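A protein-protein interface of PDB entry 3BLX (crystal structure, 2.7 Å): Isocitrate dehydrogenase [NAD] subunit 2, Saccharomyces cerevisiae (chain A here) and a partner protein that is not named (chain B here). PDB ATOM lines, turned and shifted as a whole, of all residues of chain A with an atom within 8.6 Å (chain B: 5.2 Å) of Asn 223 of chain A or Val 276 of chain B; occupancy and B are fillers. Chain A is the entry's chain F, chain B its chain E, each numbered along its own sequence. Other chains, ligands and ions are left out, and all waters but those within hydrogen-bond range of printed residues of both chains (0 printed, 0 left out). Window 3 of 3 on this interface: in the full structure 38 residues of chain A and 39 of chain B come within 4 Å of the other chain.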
ATOM      1  N   VAL A 187       3.398  -3.661  38.153  1.00  0.00           N
ATOM      2  CA  VAL A 187       2.235  -3.690  37.271  1.00  0.00           C
ATOM      3  C   VAL A 187       1.333  -2.446  37.420  1.00  0.00           C
ATOM      4  O   VAL A 187       0.988  -2.037  38.515  1.00  0.00           O
ATOM      5  CB  VAL A 187       1.403  -4.946  37.537  1.00  0.00           C
ATOM      6  CG1 VAL A 187       0.119  -4.915  36.725  1.00  0.00           C
ATOM      7  CG2 VAL A 187       2.229  -6.180  37.221  1.00  0.00           C
ATOM      8  N   HIS A 188       0.933  -1.870  36.302  1.00  0.00           N
ATOM      9  CA  HIS A 188       0.166  -0.633  36.311  1.00  0.00           C
ATOM     10  C   HIS A 188      -0.727  -0.547  35.061  1.00  0.00           C
ATOM     11  O   HIS A 188      -0.679  -1.423  34.204  1.00  0.00           O
ATOM     12  CB  HIS A 188       1.138   0.538  36.311  1.00  0.00           C
ATOM     13  CG  HIS A 188       1.986   0.604  35.079  1.00  0.00           C
ATOM     14  ND1 HIS A 188       1.791   1.540  34.089  1.00  0.00           N
ATOM     15  CD2 HIS A 188       3.017  -0.168  34.668  1.00  0.00           C
ATOM     16  CE1 HIS A 188       2.677   1.351  33.126  1.00  0.00           C
ATOM     17  NE2 HIS A 188       3.431   0.319  33.451  1.00  0.00           N
ATOM     18  N   LYS A 189      -1.537   0.507  34.969  1.00  0.00           N
ATOM     19  CA  LYS A 189      -2.387   0.752  33.806  1.00  0.00           C
ATOM     20  C   LYS A 189      -1.857   1.988  33.031  1.00  0.00           C
ATOM     21  O   LYS A 189      -1.089   2.777  33.577  1.00  0.00           O
ATOM     22  CB  LYS A 189      -3.852   0.892  34.242  1.00  0.00           C
ATOM     23  CG  LYS A 189      -4.849   0.138  33.371  1.00  0.00           C
ATOM     24  CD  LYS A 189      -4.487   0.258  31.874  1.00  0.00           C
ATOM     25  CE  LYS A 189      -5.708   0.238  30.956  1.00  0.00           C
ATOM     26  NZ  LYS A 189      -6.460  -1.038  31.064  1.00  0.00           N
ATOM     27  N   THR A 218       8.851  -2.682  34.384  1.00  0.00           N
ATOM     28  CA  THR A 218       7.462  -2.242  34.450  1.00  0.00           C
ATOM     29  C   THR A 218       6.636  -2.952  33.369  1.00  0.00           C
ATOM     30  O   THR A 218       7.144  -3.255  32.290  1.00  0.00           O
ATOM     31  CB  THR A 218       7.328  -0.704  34.311  1.00  0.00           C
ATOM     32  OG1 THR A 218       7.715  -0.293  32.993  1.00  0.00           O
ATOM     33  CG2 THR A 218       8.183   0.014  35.345  1.00  0.00           C
ATOM     34  N   GLU A 219       5.371  -3.231  33.670  1.00  0.00           N
ATOM     35  CA  GLU A 219       4.480  -3.891  32.719  1.00  0.00           C
ATOM     36  C   GLU A 219       3.029  -3.383  32.805  1.00  0.00           C
ATOM     37  O   GLU A 219       2.485  -3.172  33.896  1.00  0.00           O
ATOM     38  CB  GLU A 219       4.522  -5.404  32.929  1.00  0.00           C
ATOM     39  CG  GLU A 219       4.388  -6.240  31.662  1.00  0.00           C
ATOM     40  CD  GLU A 219       4.969  -7.660  31.821  1.00  0.00           C
ATOM     41  OE1 GLU A 219       5.143  -8.135  32.972  1.00  0.00           O
ATOM     42  OE2 GLU A 219       5.250  -8.306  30.786  1.00  0.00           O
ATOM     43  N   LEU A 220       2.398  -3.185  31.648  1.00  0.00           N
ATOM     44  CA  LEU A 220       0.968  -2.884  31.609  1.00  0.00           C
ATOM     45  C   LEU A 220       0.236  -4.081  32.136  1.00  0.00           C
ATOM     46  O   LEU A 220       0.507  -5.189  31.722  1.00  0.00           O
ATOM     47  CB  LEU A 220       0.486  -2.618  30.184  1.00  0.00           C
ATOM     48  CG  LEU A 220       0.824  -1.282  29.529  1.00  0.00           C
ATOM     49  CD1 LEU A 220       0.065  -1.144  28.217  1.00  0.00           C
ATOM     50  CD2 LEU A 220       0.487  -0.150  30.475  1.00  0.00           C
ATOM     51  N   ILE A 221      -0.705  -3.857  33.040  1.00  0.00           N
ATOM     52  CA  ILE A 221      -1.514  -4.940  33.561  1.00  0.00           C
ATOM     53  C   ILE A 221      -2.175  -5.791  32.453  1.00  0.00           C
ATOM     54  O   ILE A 221      -2.317  -6.991  32.603  1.00  0.00           O
ATOM     55  CB  ILE A 221      -2.568  -4.410  34.517  1.00  0.00           C
ATOM     56  CG1 ILE A 221      -3.286  -5.576  35.189  1.00  0.00           C
ATOM     57  CG2 ILE A 221      -3.556  -3.520  33.778  1.00  0.00           C
ATOM     58  CD1 ILE A 221      -4.433  -5.144  36.038  1.00  0.00           C
ATOM     59  N   ASP A 222      -2.558  -5.160  31.347  1.00  0.00           N
ATOM     60  CA  ASP A 222      -3.038  -5.874  30.171  1.00  0.00           C
ATOM     61  C   ASP A 222      -2.078  -6.984  29.752  1.00  0.00           C
ATOM     62  O   ASP A 222      -2.478  -8.147  29.655  1.00  0.00           O
ATOM     63  CB  ASP A 222      -3.183  -4.924  28.956  1.00  0.00           C
ATOM     64  CG  ASP A 222      -4.134  -3.742  29.205  1.00  0.00           C
ATOM     65  OD1 ASP A 222      -4.125  -3.169  30.325  1.00  0.00           O
ATOM     66  OD2 ASP A 222      -4.868  -3.364  28.254  1.00  0.00           O
ATOM     67  N   ASN A 223      -0.826  -6.604  29.476  1.00  0.00           N
ATOM     68  CA  ASN A 223       0.223  -7.540  29.054  1.00  0.00           C
ATOM     69  C   ASN A 223       0.540  -8.601  30.087  1.00  0.00           C
ATOM     70  O   ASN A 223       0.732  -9.763  29.734  1.00  0.00           O
ATOM     71  CB  ASN A 223       1.504  -6.790  28.700  1.00  0.00           C
ATOM     72  CG  ASN A 223       1.297  -5.801  27.560  1.00  0.00           C
ATOM     73  OD1 ASN A 223       0.466  -6.028  26.682  1.00  0.00           O
ATOM     74  ND2 ASN A 223       2.034  -4.694  27.582  1.00  0.00           N
ATOM     75  N   SER A 224       0.590  -8.205  31.358  1.00  0.00           N
ATOM     76  CA  SER A 224       0.807  -9.154  32.428  1.00  0.00           C
ATOM     77  C   SER A 224      -0.223 -10.274  32.437  1.00  0.00           C
ATOM     78  O   SER A 224       0.140 -11.436  32.509  1.00  0.00           O
ATOM     79  CB  SER A 224       0.840  -8.456  33.778  1.00  0.00           C
ATOM     80  OG  SER A 224       1.957  -7.583  33.835  1.00  0.00           O
ATOM     81  N   VAL A 225      -1.507  -9.954  32.353  1.00  0.00           N
ATOM     82  CA  VAL A 225      -2.454 -11.050  32.445  1.00  0.00           C
ATOM     83  C   VAL A 225      -2.418 -11.924  31.196  1.00  0.00           C
ATOM     84  O   VAL A 225      -2.691 -13.115  31.266  1.00  0.00           O
ATOM     85  CB  VAL A 225      -3.909 -10.648  32.886  1.00  0.00           C
ATOM     86  CG1 VAL A 225      -3.946  -9.290  33.519  1.00  0.00           C
ATOM     87  CG2 VAL A 225      -4.880 -10.751  31.747  1.00  0.00           C
ATOM     88  N   LEU A 226      -2.038 -11.342  30.066  1.00  0.00           N
ATOM     89  CA  LEU A 226      -1.918 -12.118  28.834  1.00  0.00           C
ATOM     90  C   LEU A 226      -0.756 -13.110  28.933  1.00  0.00           C
ATOM     91  O   LEU A 226      -0.929 -14.293  28.641  1.00  0.00           O
ATOM     92  CB  LEU A 226      -1.722 -11.192  27.631  1.00  0.00           C
ATOM     93  CG  LEU A 226      -2.186 -11.635  26.250  1.00  0.00           C
ATOM     94  CD1 LEU A 226      -1.015 -11.416  25.337  1.00  0.00           C
ATOM     95  CD2 LEU A 226      -2.608 -13.087  26.205  1.00  0.00           C
ATOM     96  N   LYS A 227       0.412 -12.616  29.344  1.00  0.00           N
ATOM     97  CA  LYS A 227       1.605 -13.448  29.538  1.00  0.00           C
ATOM     98  C   LYS A 227       1.420 -14.522  30.618  1.00  0.00           C
ATOM     99  O   LYS A 227       1.593 -15.713  30.341  1.00  0.00           O
ATOM    100  CB  LYS A 227       2.825 -12.608  29.894  1.00  0.00           C
ATOM    101  CG  LYS A 227       3.298 -11.674  28.804  1.00  0.00           C
ATOM    102  CD  LYS A 227       4.651 -11.088  29.177  1.00  0.00           C
ATOM    103  CE  LYS A 227       5.174 -10.130  28.107  1.00  0.00           C
ATOM    104  NZ  LYS A 227       6.566  -9.665  28.407  1.00  0.00           N
ATOM    105  N   VAL A 228       1.070 -14.105  31.836  1.00  0.00           N
ATOM    106  CA  VAL A 228       0.925 -15.029  32.966  1.00  0.00           C
ATOM    107  C   VAL A 228      -0.058 -16.171  32.698  1.00  0.00           C
ATOM    108  O   VAL A 228       0.136 -17.267  33.188  1.00  0.00           O
ATOM    109  CB  VAL A 228       0.465 -14.305  34.265  1.00  0.00           C
ATOM    110  CG1 VAL A 228       0.369 -15.287  35.414  1.00  0.00           C
ATOM    111  CG2 VAL A 228       1.418 -13.185  34.635  1.00  0.00           C
ATOM    112  N   VAL A 229      -1.120 -15.928  31.941  1.00  0.00           N
ATOM    113  CA  VAL A 229      -2.082 -16.993  31.716  1.00  0.00           C
ATOM    114  C   VAL A 229      -1.610 -17.952  30.627  1.00  0.00           C
ATOM    115  O   VAL A 229      -1.863 -19.165  30.705  1.00  0.00           O
ATOM    116  CB  VAL A 229      -3.490 -16.453  31.408  1.00  0.00           C
ATOM    117  CG1 VAL A 229      -4.407 -17.573  30.920  1.00  0.00           C
ATOM    118  CG2 VAL A 229      -4.070 -15.724  32.648  1.00  0.00           C
ATOM    119  N   THR A 230      -0.921 -17.435  29.612  1.00  0.00           N
ATOM    120  CA  THR A 230      -0.442 -18.322  28.541  1.00  0.00           C
ATOM    121  C   THR A 230       0.737 -19.128  29.086  1.00  0.00           C
ATOM    122  O   THR A 230       0.899 -20.302  28.761  1.00  0.00           O
ATOM    123  CB  THR A 230      -0.039 -17.599  27.210  1.00  0.00           C
ATOM    124  OG1 THR A 230       0.767 -16.462  27.502  1.00  0.00           O
ATOM    125  CG2 THR A 230      -1.256 -17.134  26.420  1.00  0.00           C
ATOM    126  N   TYR A 235       7.134 -16.145  35.194  1.00  0.00           N
ATOM    127  CA  TYR A 235       7.146 -15.153  36.271  1.00  0.00           C
ATOM    128  C   TYR A 235       7.646 -15.712  37.607  1.00  0.00           C
ATOM    129  O   TYR A 235       7.627 -15.013  38.625  1.00  0.00           O
ATOM    130  CB  TYR A 235       5.744 -14.547  36.462  1.00  0.00           C
ATOM    131  CG  TYR A 235       5.350 -13.527  35.415  1.00  0.00           C
ATOM    132  CD1 TYR A 235       4.718 -13.914  34.230  1.00  0.00           C
ATOM    133  CD2 TYR A 235       5.610 -12.181  35.607  1.00  0.00           C
ATOM    134  CE1 TYR A 235       4.364 -12.988  33.274  1.00  0.00           C
ATOM    135  CE2 TYR A 235       5.256 -11.253  34.654  1.00  0.00           C
ATOM    136  CZ  TYR A 235       4.632 -11.661  33.493  1.00  0.00           C
ATOM    137  OH  TYR A 235       4.281 -10.726  32.560  1.00  0.00           O
ATOM    138  N   GLN B  87      -3.602   0.493  22.840  1.00  0.00           N
ATOM    139  CA  GLN B  87      -3.924  -0.817  23.408  1.00  0.00           C
ATOM    140  C   GLN B  87      -4.828  -0.756  24.653  1.00  0.00           C
ATOM    141  O   GLN B  87      -5.494  -1.734  24.999  1.00  0.00           O
ATOM    142  CB  GLN B  87      -2.635  -1.590  23.717  1.00  0.00           C
ATOM    143  CG  GLN B  87      -1.749  -1.835  22.491  1.00  0.00           C
ATOM    144  CD  GLN B  87      -0.404  -2.466  22.835  1.00  0.00           C
ATOM    145  OE1 GLN B  87      -0.045  -2.601  24.011  1.00  0.00           O
ATOM    146  NE2 GLN B  87       0.346  -2.854  21.803  1.00  0.00           N
ATOM    147  N   ASN B 245      -8.117  -9.861  28.283  1.00  0.00           N
ATOM    148  CA  ASN B 245      -6.820 -10.463  28.141  1.00  0.00           C
ATOM    149  C   ASN B 245      -6.751 -11.902  28.609  1.00  0.00           C
ATOM    150  O   ASN B 245      -5.973 -12.676  28.069  1.00  0.00           O
ATOM    151  CB  ASN B 245      -5.751  -9.580  28.742  1.00  0.00           C
ATOM    152  CG  ASN B 245      -5.355  -8.447  27.794  1.00  0.00           C
ATOM    153  OD1 ASN B 245      -4.915  -8.684  26.657  1.00  0.00           O
ATOM    154  ND2 ASN B 245      -5.534  -7.217  28.241  1.00  0.00           N
ATOM    155  N   PRO B 254      -3.871 -12.676  21.182  1.00  0.00           N
ATOM    156  CA  PRO B 254      -4.521 -11.484  20.641  1.00  0.00           C
ATOM    157  C   PRO B 254      -4.751 -11.582  19.148  1.00  0.00           C
ATOM    158  O   PRO B 254      -5.666 -10.951  18.640  1.00  0.00           O
ATOM    159  CB  PRO B 254      -3.485 -10.379  20.884  1.00  0.00           C
ATOM    160  CG  PRO B 254      -2.543 -10.919  21.862  1.00  0.00           C
ATOM    161  CD  PRO B 254      -2.515 -12.383  21.671  1.00  0.00           C
ATOM    162  N   SER B 273      -8.480  -7.275  21.043  1.00  0.00           N
ATOM    163  CA  SER B 273      -7.501  -7.231  22.119  1.00  0.00           C
ATOM    164  C   SER B 273      -6.470  -6.147  21.920  1.00  0.00           C
ATOM    165  O   SER B 273      -5.594  -5.959  22.759  1.00  0.00           O
ATOM    166  CB  SER B 273      -6.815  -8.585  22.292  1.00  0.00           C
ATOM    167  OG  SER B 273      -7.453  -9.319  23.315  1.00  0.00           O
ATOM    168  N   ARG B 274      -6.571  -5.430  20.809  1.00  0.00           N
ATOM    169  CA  ARG B 274      -5.604  -4.392  20.485  1.00  0.00           C
ATOM    170  C   ARG B 274      -4.189  -4.957  20.311  1.00  0.00           C
ATOM    171  O   ARG B 274      -3.209  -4.235  20.464  1.00  0.00           O
ATOM    172  CB  ARG B 274      -5.638  -3.291  21.547  1.00  0.00           C
ATOM    173  CG  ARG B 274      -6.650  -2.188  21.263  1.00  0.00           C
ATOM    174  CD  ARG B 274      -8.093  -2.590  21.538  1.00  0.00           C
ATOM    175  NE  ARG B 274      -9.027  -1.516  21.183  1.00  0.00           N
ATOM    176  CZ  ARG B 274      -9.393  -0.528  22.002  1.00  0.00           C
ATOM    177  NH1 ARG B 274      -8.903  -0.479  23.237  1.00  0.00           N
ATOM    178  NH2 ARG B 274     -10.249   0.412  21.587  1.00  0.00           N
ATOM    179  N   HIS B 275      -4.103  -6.249  19.980  1.00  0.00           N
ATOM    180  CA  HIS B 275      -2.831  -6.953  19.757  1.00  0.00           C
ATOM    181  C   HIS B 275      -1.838  -6.712  20.888  1.00  0.00           C
ATOM    182  O   HIS B 275      -0.627  -6.592  20.678  1.00  0.00           O
ATOM    183  CB  HIS B 275      -2.217  -6.562  18.412  1.00  0.00           C
ATOM    184  CG  HIS B 275      -2.769  -7.323  17.243  1.00  0.00           C
ATOM    185  ND1 HIS B 275      -1.965  -8.005  16.349  1.00  0.00           N
ATOM    186  CD2 HIS B 275      -4.043  -7.504  16.815  1.00  0.00           C
ATOM    187  CE1 HIS B 275      -2.722  -8.573  15.423  1.00  0.00           C
ATOM    188  NE2 HIS B 275      -3.985  -8.281  15.679  1.00  0.00           N
ATOM    189  N   VAL B 276      -2.400  -6.616  22.082  1.00  0.00           N
ATOM    190  CA  VAL B 276      -1.652  -6.443  23.310  1.00  0.00           C
ATOM    191  C   VAL B 276      -0.304  -7.181  23.260  1.00  0.00           C
ATOM    192  O   VAL B 276       0.744  -6.566  23.004  1.00  0.00           O
ATOM    193  CB  VAL B 276      -2.512  -6.898  24.532  1.00  0.00           C
ATOM    194  CG1 VAL B 276      -3.307  -5.705  25.143  1.00  0.00           C
ATOM    195  CG2 VAL B 276      -3.451  -8.050  24.126  1.00  0.00           C
ATOM    196  N   GLY B 277      -0.339  -8.495  23.481  1.00  0.00           N
ATOM    197  CA  GLY B 277       0.875  -9.296  23.497  1.00  0.00           C
ATOM    198  C   GLY B 277       1.293  -9.789  22.120  1.00  0.00           C
ATOM    199  O   GLY B 277       2.050 -10.769  22.005  1.00  0.00           O
ATOM    200  N   LEU B 278       0.780  -9.122  21.081  1.00  0.00           N
ATOM    201  CA  LEU B 278       1.245  -9.342  19.712  1.00  0.00           C
ATOM    202  C   LEU B 278       2.503  -8.529  19.464  1.00  0.00           C
ATOM    203  O   LEU B 278       2.491  -7.533  18.727  1.00  0.00           O
ATOM    204  CB  LEU B 278       0.166  -9.035  18.670  1.00  0.00           C
ATOM    205  CG  LEU B 278      -0.402 -10.285  17.982  1.00  0.00           C
ATOM    206  CD1 LEU B 278       0.245 -10.509  16.612  1.00  0.00           C
ATOM    207  CD2 LEU B 278      -0.285 -11.556  18.865  1.00  0.00           C
ATOM    208  N   ASP B 279       3.573  -8.965  20.133  1.00  0.00           N
ATOM    209  CA  ASP B 279       4.929  -8.513  19.861  1.00  0.00           C
ATOM    210  C   ASP B 279       5.303  -9.101  18.501  1.00  0.00           C
ATOM    211  O   ASP B 279       4.931  -8.547  17.445  1.00  0.00           O
ATOM    212  CB  ASP B 279       5.925  -9.013  20.927  1.00  0.00           C
ATOM    213  CG  ASP B 279       5.397  -8.884  22.358  1.00  0.00           C
ATOM    214  OD1 ASP B 279       4.166  -8.757  22.550  1.00  0.00           O
ATOM    215  OD2 ASP B 279       6.227  -8.926  23.301  1.00  0.00           O
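Thr 218 of chain A touches none of the printed residues of chain B. Printed residues of chain B within 4 Å of Asp 222 of chain A: Gln 87, Asn 245 and Val 276. Of chain B, only Val 276 (3.7 Å) comes within 4 Å of Asn 223 of chain A. Printed residues of chain B within 4 Å of Val 225 of chain A: Asn 245. Of the printed residues of chain B, Leu 226 of chain A touches Asn 245 (3.9 Å), Pro 254 (3.8 Å) and Gly 277 (3.4 Å). Printed residues of chain A within 4 Å of Asn 245 of chain B: Asp 222, Val 225 and Leu 226. Of the printed residues of chain A, Pro 254 of chain B touches Leu 226. Ser 273 of chain B touches none of the printed residues of chain A. Val 276 of chain B touches just these residues of chain A: Asp 222 (3.9 Å) and Asn 223 (3.7 Å). Gly 277 of chain B touches one residue of chain A. The nearest residue of chain B that does not touch Asn 223 of chain A is Gly 277 of chain B (4.1 Å). The nearest printed residue of chain A that does not touch Gln 87 of chain B is Asn 223 of chain A (4.4 Å).
OD1 of Asp 222 of chain A lies within salt-bridge range of NZ of Lys 189 of chain A, at 3.2 Å. The backbone carbonyl oxygen (O) of Leu 226 of chain A lies within hydrogen-bond range of the side-chain hydroxyl (OG1) of Thr 230 of chain A, 3.0 Å away.
Hydrophobic or aromatic side chains of chain A that line the printed part of chain B: Val 225 and Leu 226. Along chain A the printed residues that touch a printed residue of chain B span positions 222 to 226. Printed residues of chain B that touch a printed residue of chain A: Gln 87, Asn 245, Pro 254, Val 276 and Gly 277. Hydrophobic or aromatic side chains of chain B that line the printed part of chain A: Pro 254 and Val 276. Along chain B the printed residues that touch a printed residue of chain A span positions 87 to 277. Among the printed residues, no Asp or Glu carboxylate lies within 4 Å of a Lys or Arg side-chain nitrogen of the other chain.
Among the printed residues, pairs that only touch across the chains: Val 225 of chain A with Asn 245 of chain B, Leu 226 of chain A with Gly 277 of chain B, Asn 223 of chain A with Val 276 of chain B, Asp 222 of chain A with Gln 87 of chain B, Leu 226 of chain A with Pro 254 of chain B, Leu 226 of chain A with Asn 245 of chain B and Asp 222 of chain A with Val 276 of chain B.
O of Asp 222 of chain A sits close to ND2 of Asn 245 of chain B (3.5 Å).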
